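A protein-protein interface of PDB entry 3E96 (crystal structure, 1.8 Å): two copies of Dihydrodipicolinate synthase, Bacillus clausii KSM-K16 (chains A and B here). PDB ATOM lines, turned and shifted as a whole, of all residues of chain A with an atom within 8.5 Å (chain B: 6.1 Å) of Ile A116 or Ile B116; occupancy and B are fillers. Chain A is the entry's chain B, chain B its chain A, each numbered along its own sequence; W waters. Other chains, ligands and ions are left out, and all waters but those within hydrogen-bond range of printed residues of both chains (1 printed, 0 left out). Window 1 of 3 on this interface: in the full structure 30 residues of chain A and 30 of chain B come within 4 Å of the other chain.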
ATOM      1  N   ASN A  55     -14.643 -38.247  -2.001  1.00  0.00           N
ATOM      2  CA  ASN A  55     -16.073 -38.126  -1.768  1.00  0.00           C
ATOM      3  C   ASN A  55     -16.755 -39.471  -1.561  1.00  0.00           C
ATOM      4  O   ASN A  55     -17.763 -39.549  -0.867  1.00  0.00           O
ATOM      5  CB  ASN A  55     -16.729 -37.322  -2.890  1.00  0.00           C
ATOM      6  CG  ASN A  55     -16.737 -35.828  -2.589  1.00  0.00           C
ATOM      7  OD1 ASN A  55     -16.542 -35.004  -3.477  1.00  0.00           O
ATOM      8  ND2 ASN A  55     -16.968 -35.475  -1.321  1.00  0.00           N
ATOM      9  N   PHE A  59     -16.120 -37.857   2.850  1.00  0.00           N
ATOM     10  CA  PHE A  59     -15.257 -36.858   3.469  1.00  0.00           C
ATOM     11  C   PHE A  59     -16.002 -35.804   4.292  1.00  0.00           C
ATOM     12  O   PHE A  59     -15.644 -35.529   5.442  1.00  0.00           O
ATOM     13  CB  PHE A  59     -14.440 -36.175   2.367  1.00  0.00           C
ATOM     14  CG  PHE A  59     -13.645 -34.995   2.833  1.00  0.00           C
ATOM     15  CD1 PHE A  59     -12.603 -35.153   3.734  1.00  0.00           C
ATOM     16  CD2 PHE A  59     -13.919 -33.722   2.336  1.00  0.00           C
ATOM     17  CE1 PHE A  59     -11.838 -34.064   4.137  1.00  0.00           C
ATOM     18  CE2 PHE A  59     -13.162 -32.626   2.732  1.00  0.00           C
ATOM     19  CZ  PHE A  59     -12.116 -32.798   3.635  1.00  0.00           C
ATOM     20  N   TYR A  60     -17.039 -35.209   3.711  1.00  0.00           N
ATOM     21  CA  TYR A  60     -17.784 -34.167   4.405  1.00  0.00           C
ATOM     22  C   TYR A  60     -18.593 -34.629   5.611  1.00  0.00           C
ATOM     23  O   TYR A  60     -19.093 -33.804   6.378  1.00  0.00           O
ATOM     24  CB  TYR A  60     -18.669 -33.422   3.408  1.00  0.00           C
ATOM     25  CG  TYR A  60     -17.841 -32.620   2.428  1.00  0.00           C
ATOM     26  CD1 TYR A  60     -17.033 -31.575   2.872  1.00  0.00           C
ATOM     27  CD2 TYR A  60     -17.833 -32.928   1.068  1.00  0.00           C
ATOM     28  CE1 TYR A  60     -16.235 -30.855   1.990  1.00  0.00           C
ATOM     29  CE2 TYR A  60     -17.036 -32.212   0.173  1.00  0.00           C
ATOM     30  CZ  TYR A  60     -16.240 -31.175   0.646  1.00  0.00           C
ATOM     31  OH  TYR A  60     -15.460 -30.452  -0.227  1.00  0.00           O
ATOM     32  N   ALA A  61     -18.712 -35.942   5.785  1.00  0.00           N
ATOM     33  CA  ALA A  61     -19.440 -36.488   6.933  1.00  0.00           C
ATOM     34  C   ALA A  61     -18.454 -36.793   8.065  1.00  0.00           C
ATOM     35  O   ALA A  61     -18.841 -37.253   9.143  1.00  0.00           O
ATOM     36  CB  ALA A  61     -20.181 -37.758   6.527  1.00  0.00           C
ATOM     37  N   GLY A  89      -9.875 -30.069   1.978  1.00  0.00           N
ATOM     38  CA  GLY A  89     -10.840 -29.066   1.551  1.00  0.00           C
ATOM     39  C   GLY A  89     -11.178 -28.037   2.619  1.00  0.00           C
ATOM     40  O   GLY A  89     -10.409 -27.852   3.561  1.00  0.00           O
ATOM     41  N   TYR A  90     -12.330 -27.381   2.458  1.00  0.00           N
ATOM     42  CA  TYR A  90     -12.828 -26.350   3.374  1.00  0.00           C
ATOM     43  C   TYR A  90     -12.111 -25.010   3.184  1.00  0.00           C
ATOM     44  O   TYR A  90     -11.540 -24.758   2.126  1.00  0.00           O
ATOM     45  CB  TYR A  90     -12.699 -26.818   4.827  1.00  0.00           C
ATOM     46  CG  TYR A  90     -13.494 -28.069   5.127  1.00  0.00           C
ATOM     47  CD1 TYR A  90     -14.886 -28.078   5.014  1.00  0.00           C
ATOM     48  CD2 TYR A  90     -12.858 -29.244   5.534  1.00  0.00           C
ATOM     49  CE1 TYR A  90     -15.625 -29.223   5.301  1.00  0.00           C
ATOM     50  CE2 TYR A  90     -13.588 -30.396   5.827  1.00  0.00           C
ATOM     51  CZ  TYR A  90     -14.970 -30.377   5.708  1.00  0.00           C
ATOM     52  OH  TYR A  90     -15.697 -31.512   6.005  1.00  0.00           O
ATOM     53  N   ALA A  91     -12.157 -24.149   4.197  1.00  0.00           N
ATOM     54  CA  ALA A  91     -11.494 -22.849   4.114  1.00  0.00           C
ATOM     55  C   ALA A  91     -10.015 -23.070   3.794  1.00  0.00           C
ATOM     56  O   ALA A  91      -9.442 -24.088   4.185  1.00  0.00           O
ATOM     57  CB  ALA A  91     -11.647 -22.100   5.439  1.00  0.00           C
ATOM     58  N   HIS A 113     -10.398 -30.879  -2.956  1.00  0.00           N
ATOM     59  CA  HIS A 113     -11.792 -30.962  -3.374  1.00  0.00           C
ATOM     60  C   HIS A 113     -12.211 -29.626  -3.953  1.00  0.00           C
ATOM     61  O   HIS A 113     -11.576 -28.604  -3.701  1.00  0.00           O
ATOM     62  CB  HIS A 113     -12.701 -31.259  -2.178  1.00  0.00           C
ATOM     63  CG  HIS A 113     -12.715 -32.697  -1.769  1.00  0.00           C
ATOM     64  ND1 HIS A 113     -13.433 -33.655  -2.449  1.00  0.00           N
ATOM     65  CD2 HIS A 113     -12.084 -33.342  -0.760  1.00  0.00           C
ATOM     66  CE1 HIS A 113     -13.243 -34.832  -1.876  1.00  0.00           C
ATOM     67  NE2 HIS A 113     -12.428 -34.668  -0.849  1.00  0.00           N
ATOM     68  N   MET A 114     -13.281 -29.638  -4.739  1.00  0.00           N
ATOM     69  CA  MET A 114     -13.806 -28.403  -5.295  1.00  0.00           C
ATOM     70  C   MET A 114     -14.355 -27.686  -4.064  1.00  0.00           C
ATOM     71  O   MET A 114     -15.001 -28.309  -3.223  1.00  0.00           O
ATOM     72  CB  MET A 114     -14.949 -28.708  -6.271  1.00  0.00           C
ATOM     73  CG  MET A 114     -15.489 -27.492  -7.021  1.00  0.00           C
ATOM     74  SD  MET A 114     -14.350 -26.898  -8.310  1.00  0.00           S
ATOM     75  CE  MET A 114     -15.014 -25.139  -8.582  1.00  0.00           C
ATOM     76  N   PRO A 115     -14.091 -26.377  -3.923  1.00  0.00           N
ATOM     77  CA  PRO A 115     -14.621 -25.689  -2.741  1.00  0.00           C
ATOM     78  C   PRO A 115     -16.148 -25.808  -2.678  1.00  0.00           C
ATOM     79  O   PRO A 115     -16.819 -25.758  -3.709  1.00  0.00           O
ATOM     80  CB  PRO A 115     -14.138 -24.247  -2.934  1.00  0.00           C
ATOM     81  CG  PRO A 115     -13.982 -24.121  -4.439  1.00  0.00           C
ATOM     82  CD  PRO A 115     -13.364 -25.448  -4.803  1.00  0.00           C
ATOM     83  N   ILE A 116     -16.696 -25.976  -1.476  1.00  0.00           N
ATOM     84  CA  ILE A 116     -18.142 -26.110  -1.343  1.00  0.00           C
ATOM     85  C   ILE A 116     -18.885 -24.810  -1.047  1.00  0.00           C
ATOM     86  O   ILE A 116     -20.092 -24.827  -0.810  1.00  0.00           O
ATOM     87  CB  ILE A 116     -18.529 -27.178  -0.271  1.00  0.00           C
ATOM     88  CG1 ILE A 116     -17.673 -27.026   0.990  1.00  0.00           C
ATOM     89  CG2 ILE A 116     -18.365 -28.576  -0.858  1.00  0.00           C
ATOM     90  CD1 ILE A 116     -17.922 -25.752   1.771  1.00  0.00           C
ATOM     91  N   HIS A 117     -18.176 -23.685  -1.076  1.00  0.00           N
ATOM     92  CA  HIS A 117     -18.812 -22.392  -0.815  1.00  0.00           C
ATOM     93  C   HIS A 117     -19.945 -22.167  -1.816  1.00  0.00           C
ATOM     94  O   HIS A 117     -19.784 -22.436  -3.007  1.00  0.00           O
ATOM     95  CB  HIS A 117     -17.796 -21.252  -0.965  1.00  0.00           C
ATOM     96  CG  HIS A 117     -16.519 -21.463  -0.212  1.00  0.00           C
ATOM     97  ND1 HIS A 117     -15.705 -22.555  -0.416  1.00  0.00           N
ATOM     98  CD2 HIS A 117     -15.891 -20.693   0.710  1.00  0.00           C
ATOM     99  CE1 HIS A 117     -14.630 -22.451   0.343  1.00  0.00           C
ATOM    100  NE2 HIS A 117     -14.717 -21.329   1.037  1.00  0.00           N
ATOM    101  N   PRO A 118     -21.107 -21.668  -1.355  1.00  0.00           N
ATOM    102  CA  PRO A 118     -22.216 -21.435  -2.287  1.00  0.00           C
ATOM    103  C   PRO A 118     -21.902 -20.343  -3.308  1.00  0.00           C
ATOM    104  O   PRO A 118     -22.516 -20.279  -4.376  1.00  0.00           O
ATOM    105  CB  PRO A 118     -23.370 -21.045  -1.367  1.00  0.00           C
ATOM    106  CG  PRO A 118     -22.678 -20.419  -0.199  1.00  0.00           C
ATOM    107  CD  PRO A 118     -21.513 -21.351   0.025  1.00  0.00           C
ATOM    108  N   TYR A 119     -20.954 -19.473  -2.972  1.00  0.00           N
ATOM    109  CA  TYR A 119     -20.577 -18.398  -3.877  1.00  0.00           C
ATOM    110  C   TYR A 119     -19.140 -18.577  -4.336  1.00  0.00           C
ATOM    111  O   TYR A 119     -18.210 -18.563  -3.522  1.00  0.00           O
ATOM    112  CB  TYR A 119     -20.732 -17.032  -3.197  1.00  0.00           C
ATOM    113  CG  TYR A 119     -21.971 -16.896  -2.336  1.00  0.00           C
ATOM    114  CD1 TYR A 119     -23.220 -17.312  -2.797  1.00  0.00           C
ATOM    115  CD2 TYR A 119     -21.889 -16.363  -1.051  1.00  0.00           C
ATOM    116  CE1 TYR A 119     -24.355 -17.206  -1.993  1.00  0.00           C
ATOM    117  CE2 TYR A 119     -23.010 -16.249  -0.243  1.00  0.00           C
ATOM    118  CZ  TYR A 119     -24.238 -16.672  -0.713  1.00  0.00           C
ATOM    119  OH  TYR A 119     -25.341 -16.569   0.099  1.00  0.00           O
ATOM    120  N   VAL A 120     -18.964 -18.757  -5.643  1.00  0.00           N
ATOM    121  CA  VAL A 120     -17.639 -18.924  -6.225  1.00  0.00           C
ATOM    122  C   VAL A 120     -17.561 -18.199  -7.562  1.00  0.00           C
ATOM    123  O   VAL A 120     -18.566 -18.073  -8.264  1.00  0.00           O
ATOM    124  CB  VAL A 120     -17.305 -20.415  -6.473  1.00  0.00           C
ATOM    125  CG1 VAL A 120     -17.232 -21.165  -5.149  1.00  0.00           C
ATOM    126  CG2 VAL A 120     -18.356 -21.043  -7.394  1.00  0.00           C
ATOM    127  N   TYR A 128      -8.129 -19.741  -4.867  1.00  0.00           N
ATOM    128  CA  TYR A 128      -8.355 -20.766  -3.854  1.00  0.00           C
ATOM    129  C   TYR A 128      -7.360 -21.912  -4.010  1.00  0.00           C
ATOM    130  O   TYR A 128      -6.630 -22.245  -3.077  1.00  0.00           O
ATOM    131  CB  TYR A 128      -9.782 -21.315  -3.960  1.00  0.00           C
ATOM    132  CG  TYR A 128     -10.078 -22.411  -2.962  1.00  0.00           C
ATOM    133  CD1 TYR A 128     -10.312 -22.118  -1.619  1.00  0.00           C
ATOM    134  CD2 TYR A 128     -10.089 -23.749  -3.354  1.00  0.00           C
ATOM    135  CE1 TYR A 128     -10.549 -23.132  -0.688  1.00  0.00           C
ATOM    136  CE2 TYR A 128     -10.323 -24.768  -2.439  1.00  0.00           C
ATOM    137  CZ  TYR A 128     -10.552 -24.455  -1.108  1.00  0.00           C
ATOM    138  OH  TYR A 128     -10.773 -25.469  -0.205  1.00  0.00           O
ATOM    139  N   PHE A 129      -7.330 -22.513  -5.195  1.00  0.00           N
ATOM    140  CA  PHE A 129      -6.421 -23.622  -5.450  1.00  0.00           C
ATOM    141  C   PHE A 129      -4.959 -23.186  -5.397  1.00  0.00           C
ATOM    142  O   PHE A 129      -4.121 -23.858  -4.793  1.00  0.00           O
ATOM    143  CB  PHE A 129      -6.722 -24.254  -6.811  1.00  0.00           C
ATOM    144  CG  PHE A 129      -8.002 -25.053  -6.842  1.00  0.00           C
ATOM    145  CD1 PHE A 129      -8.212 -26.089  -5.933  1.00  0.00           C
ATOM    146  CD2 PHE A 129      -8.978 -24.790  -7.796  1.00  0.00           C
ATOM    147  CE1 PHE A 129      -9.382 -26.860  -5.976  1.00  0.00           C
ATOM    148  CE2 PHE A 129     -10.150 -25.551  -7.851  1.00  0.00           C
ATOM    149  CZ  PHE A 129     -10.348 -26.589  -6.936  1.00  0.00           C
ATOM    150  N   LYS A 145     -15.149 -29.652 -10.832  1.00  0.00           N
ATOM    151  CA  LYS A 145     -16.472 -30.144 -11.204  1.00  0.00           C
ATOM    152  C   LYS A 145     -17.612 -29.151 -11.401  1.00  0.00           C
ATOM    153  O   LYS A 145     -18.742 -29.572 -11.644  1.00  0.00           O
ATOM    154  CB  LYS A 145     -16.928 -31.182 -10.178  1.00  0.00           C
ATOM    155  CG  LYS A 145     -17.271 -30.595  -8.818  1.00  0.00           C
ATOM    156  CD  LYS A 145     -17.903 -31.663  -7.939  1.00  0.00           C
ATOM    157  CE  LYS A 145     -18.463 -31.090  -6.658  1.00  0.00           C
ATOM    158  NZ  LYS A 145     -19.181 -32.150  -5.884  1.00  0.00           N
ATOM    159  N   PRO A 281     -26.016 -36.878   5.935  1.00  0.00           N
ATOM    160  CA  PRO A 281     -27.267 -36.790   5.172  1.00  0.00           C
ATOM    161  C   PRO A 281     -27.699 -37.875   4.178  1.00  0.00           C
ATOM    162  O   PRO A 281     -28.431 -37.579   3.233  1.00  0.00           O
ATOM    163  CB  PRO A 281     -27.146 -35.428   4.499  1.00  0.00           C
ATOM    164  CG  PRO A 281     -25.687 -35.387   4.150  1.00  0.00           C
ATOM    165  CD  PRO A 281     -25.030 -35.904   5.424  1.00  0.00           C
ATOM    166  N   TYR B  60     -18.242 -20.536   5.075  1.00  0.00           N
ATOM    167  CA  TYR B  60     -17.338 -21.565   4.582  1.00  0.00           C
ATOM    168  C   TYR B  60     -15.891 -21.132   4.314  1.00  0.00           C
ATOM    169  O   TYR B  60     -15.019 -21.976   4.104  1.00  0.00           O
ATOM    170  CB  TYR B  60     -17.960 -22.236   3.352  1.00  0.00           C
ATOM    171  CG  TYR B  60     -19.201 -23.036   3.713  1.00  0.00           C
ATOM    172  CD1 TYR B  60     -19.114 -24.132   4.575  1.00  0.00           C
ATOM    173  CD2 TYR B  60     -20.462 -22.672   3.239  1.00  0.00           C
ATOM    174  CE1 TYR B  60     -20.252 -24.845   4.960  1.00  0.00           C
ATOM    175  CE2 TYR B  60     -21.611 -23.379   3.621  1.00  0.00           C
ATOM    176  CZ  TYR B  60     -21.497 -24.462   4.483  1.00  0.00           C
ATOM    177  OH  TYR B  60     -22.623 -25.146   4.887  1.00  0.00           O
ATOM    178  N   TYR B  90     -21.409 -28.422   8.712  1.00  0.00           N
ATOM    179  CA  TYR B  90     -20.414 -29.483   8.561  1.00  0.00           C
ATOM    180  C   TYR B  90     -20.909 -30.815   9.115  1.00  0.00           C
ATOM    181  O   TYR B  90     -22.112 -31.006   9.310  1.00  0.00           O
ATOM    182  CB  TYR B  90     -19.098 -29.081   9.232  1.00  0.00           C
ATOM    183  CG  TYR B  90     -18.505 -27.800   8.680  1.00  0.00           C
ATOM    184  CD1 TYR B  90     -18.124 -27.703   7.337  1.00  0.00           C
ATOM    185  CD2 TYR B  90     -18.315 -26.687   9.500  1.00  0.00           C
ATOM    186  CE1 TYR B  90     -17.563 -26.525   6.831  1.00  0.00           C
ATOM    187  CE2 TYR B  90     -17.758 -25.513   9.006  1.00  0.00           C
ATOM    188  CZ  TYR B  90     -17.383 -25.439   7.675  1.00  0.00           C
ATOM    189  OH  TYR B  90     -16.823 -24.278   7.194  1.00  0.00           O
ATOM    190  N   MET B 114     -27.536 -25.819   5.280  1.00  0.00           N
ATOM    191  CA  MET B 114     -27.844 -27.108   4.767  1.00  0.00           C
ATOM    192  C   MET B 114     -26.570 -27.842   4.470  1.00  0.00           C
ATOM    193  O   MET B 114     -25.576 -27.238   4.079  1.00  0.00           O
ATOM    194  CB  MET B 114     -28.719 -27.056   3.578  1.00  0.00           C
ATOM    195  CG  MET B 114     -29.686 -28.152   3.827  1.00  0.00           C
ATOM    196  SD  MET B 114     -30.760 -28.240   2.648  1.00  0.00           S
ATOM    197  CE  MET B 114     -30.495 -29.925   1.981  1.00  0.00           C
ATOM    198  N   PRO B 115     -26.571 -29.165   4.687  1.00  0.00           N
ATOM    199  CA  PRO B 115     -25.366 -29.953   4.435  1.00  0.00           C
ATOM    200  C   PRO B 115     -24.815 -29.738   3.035  1.00  0.00           C
ATOM    201  O   PRO B 115     -25.565 -29.697   2.059  1.00  0.00           O
ATOM    202  CB  PRO B 115     -25.832 -31.386   4.693  1.00  0.00           C
ATOM    203  CG  PRO B 115     -27.293 -31.338   4.342  1.00  0.00           C
ATOM    204  CD  PRO B 115     -27.717 -30.045   4.983  1.00  0.00           C
ATOM    205  N   ILE B 116     -23.497 -29.583   2.952  1.00  0.00           N
ATOM    206  CA  ILE B 116     -22.847 -29.358   1.672  1.00  0.00           C
ATOM    207  C   ILE B 116     -22.325 -30.627   0.998  1.00  0.00           C
ATOM    208  O   ILE B 116     -21.689 -30.555  -0.054  1.00  0.00           O
ATOM    209  CB  ILE B 116     -21.693 -28.311   1.798  1.00  0.00           C
ATOM    210  CG1 ILE B 116     -20.849 -28.566   3.052  1.00  0.00           C
ATOM    211  CG2 ILE B 116     -22.281 -26.911   1.869  1.00  0.00           C
ATOM    212  CD1 ILE B 116     -20.124 -29.887   3.071  1.00  0.00           C
ATOM    213  N   HIS B 117     -22.609 -31.786   1.588  1.00  0.00           N
ATOM    214  CA  HIS B 117     -22.166 -33.059   1.022  1.00  0.00           C
ATOM    215  C   HIS B 117     -22.695 -33.177  -0.410  1.00  0.00           C
ATOM    216  O   HIS B 117     -23.824 -32.787  -0.688  1.00  0.00           O
ATOM    217  CB  HIS B 117     -22.723 -34.244   1.830  1.00  0.00           C
ATOM    218  CG  HIS B 117     -22.510 -34.135   3.308  1.00  0.00           C
ATOM    219  ND1 HIS B 117     -22.932 -33.049   4.044  1.00  0.00           N
ATOM    220  CD2 HIS B 117     -21.952 -34.995   4.192  1.00  0.00           C
ATOM    221  CE1 HIS B 117     -22.644 -33.245   5.318  1.00  0.00           C
ATOM    222  NE2 HIS B 117     -22.050 -34.419   5.435  1.00  0.00           N
ATOM    223  N   PRO B 118     -21.889 -33.731  -1.330  1.00  0.00           N
ATOM    224  CA  PRO B 118     -22.335 -33.883  -2.720  1.00  0.00           C
ATOM    225  C   PRO B 118     -23.448 -34.921  -2.848  1.00  0.00           C
ATOM    226  O   PRO B 118     -24.199 -34.910  -3.822  1.00  0.00           O
ATOM    227  CB  PRO B 118     -21.063 -34.315  -3.449  1.00  0.00           C
ATOM    228  CG  PRO B 118     -20.293 -35.044  -2.374  1.00  0.00           C
ATOM    229  CD  PRO B 118     -20.480 -34.136  -1.184  1.00  0.00           C
ATOM    230  N   TYR B 119     -23.541 -35.816  -1.865  1.00  0.00           N
ATOM    231  CA  TYR B 119     -24.572 -36.857  -1.866  1.00  0.00           C
ATOM    232  C   TYR B 119     -25.507 -36.688  -0.667  1.00  0.00           C
ATOM    233  O   TYR B 119     -25.075 -36.739   0.488  1.00  0.00           O
ATOM    234  CB  TYR B 119     -23.941 -38.259  -1.808  1.00  0.00           C
ATOM    235  CG  TYR B 119     -22.682 -38.416  -2.635  1.00  0.00           C
ATOM    236  CD1 TYR B 119     -22.592 -37.872  -3.912  1.00  0.00           C
ATOM    237  CD2 TYR B 119     -21.574 -39.099  -2.130  1.00  0.00           C
ATOM    238  CE1 TYR B 119     -21.434 -37.995  -4.668  1.00  0.00           C
ATOM    239  CE2 TYR B 119     -20.405 -39.232  -2.881  1.00  0.00           C
ATOM    240  CZ  TYR B 119     -20.345 -38.675  -4.147  1.00  0.00           C
ATOM    241  OH  TYR B 119     -19.201 -38.795  -4.904  1.00  0.00           O
ATOM    242  N   VAL B 120     -26.787 -36.469  -0.953  1.00  0.00           N
ATOM    243  CA  VAL B 120     -27.801 -36.308   0.078  1.00  0.00           C
ATOM    244  C   VAL B 120     -29.096 -36.959  -0.394  1.00  0.00           C
ATOM    245  O   VAL B 120     -29.361 -37.026  -1.593  1.00  0.00           O
ATOM    246  CB  VAL B 120     -28.102 -34.805   0.376  1.00  0.00           C
ATOM    247  CG1 VAL B 120     -26.863 -34.115   0.955  1.00  0.00           C
ATOM    248  CG2 VAL B 120     -28.557 -34.101  -0.895  1.00  0.00           C
HETATM  249  O   HOH W   1     -15.397 -24.497   4.590  1.00  0.00           O
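Water W1 lies within hydrogen-bond range of O of Tyr B60 (2.6 Å), OH of Tyr B90 (3.0 Å) and N of Ala A91 (3.3 Å).
Among the printed residues, pairs that only touch across the chains: Asn A55 with Pro B118 (3.5 Å), Asn A55 with Tyr B119 (3.3 Å), Tyr A60 with Ile B116 (3.5 Å), Tyr A60 with Pro B118 (3.7 Å), Ala A61 with His B117 (3.7 Å), Tyr A90 with Tyr B90 (3.6 Å), Ala A91 with Tyr B60 (3.6 Å), Ile A116 with Tyr B60 (3.5 Å), Ile A116 with Ile B116 (3.9 Å), Pro A118 with Tyr B60 (3.6 Å), Lys A145 with Pro B118 (3.8 Å), Pro A281 with His B117 (3.3 Å), Pro A281 with Tyr B119 (3.95 Å) and Pro A281 with Val B120 (3.5 Å).
Of the printed residues of chain B, Ile A116 touches Tyr B60 and Ile B116. Printed residues of chain B within 4 Å of Pro A118: Tyr B60 (3.6 Å). Tyr A128 touches none of the printed residues of chain B. Phe A129 touches none of the printed residues of chain B. Ile B116 touches just these residues of chain A: Tyr A60 (3.5 Å) and Ile A116 (3.9 Å). Of the printed residues of chain A, Pro B118 touches Asn A55, Tyr A60 and Lys A145. Of the printed residues of chain A, Val B120 touches Pro A281 (3.5 Å). The nearest residue of chain A that does not touch Ile B116 is Tyr A90 (5.1 Å). The nearest printed residue of chain A that does not touch His B117 is Ile A116 (5.9 Å).
Of the 19 printed residues of chain A, 10 touch a printed residue of chain B. Hydrophobic or aromatic side chains of chain A that line the printed part of chain B: Tyr A60, Ala A61, Tyr A90, Ala A91, Ile A116, His A117, Pro A118 and Pro A281. Among the printed residues, 16 pairs touch across the chains. Among the printed residues, no Asp or Glu carboxylate lies within 4 Å of a Lys or Arg side-chain nitrogen of the other chain.
O of Tyr B60 sits at hydrogen-bond distance from NE2 of His A117. The backbone carbonyl oxygen (O) of Tyr A60 sits at hydrogen-bond distance from a ring nitrogen (NE2) of His B117 (3.2 Å).
The side-chain hydroxyl of Tyr A128 sits at hydrogen-bond distance from the backbone carbonyl oxygen of Tyr A90 (2.6 Å).
Tyr A60 touches Ile B116, and with the chains exchanged Ile A116 touches Tyr B60. Tyr A60 touches Pro B118, and with the chains exchanged Pro A118 touches Tyr B60. Tyr B90 touches its own counterpart, Tyr A90. Ile B116 touches its own counterpart, Ile A116. 9 positions are printed for both chains. Of the 16 pairs that touch across the chains among the printed residues, 8 have their exchanged pair printed and touching as well.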
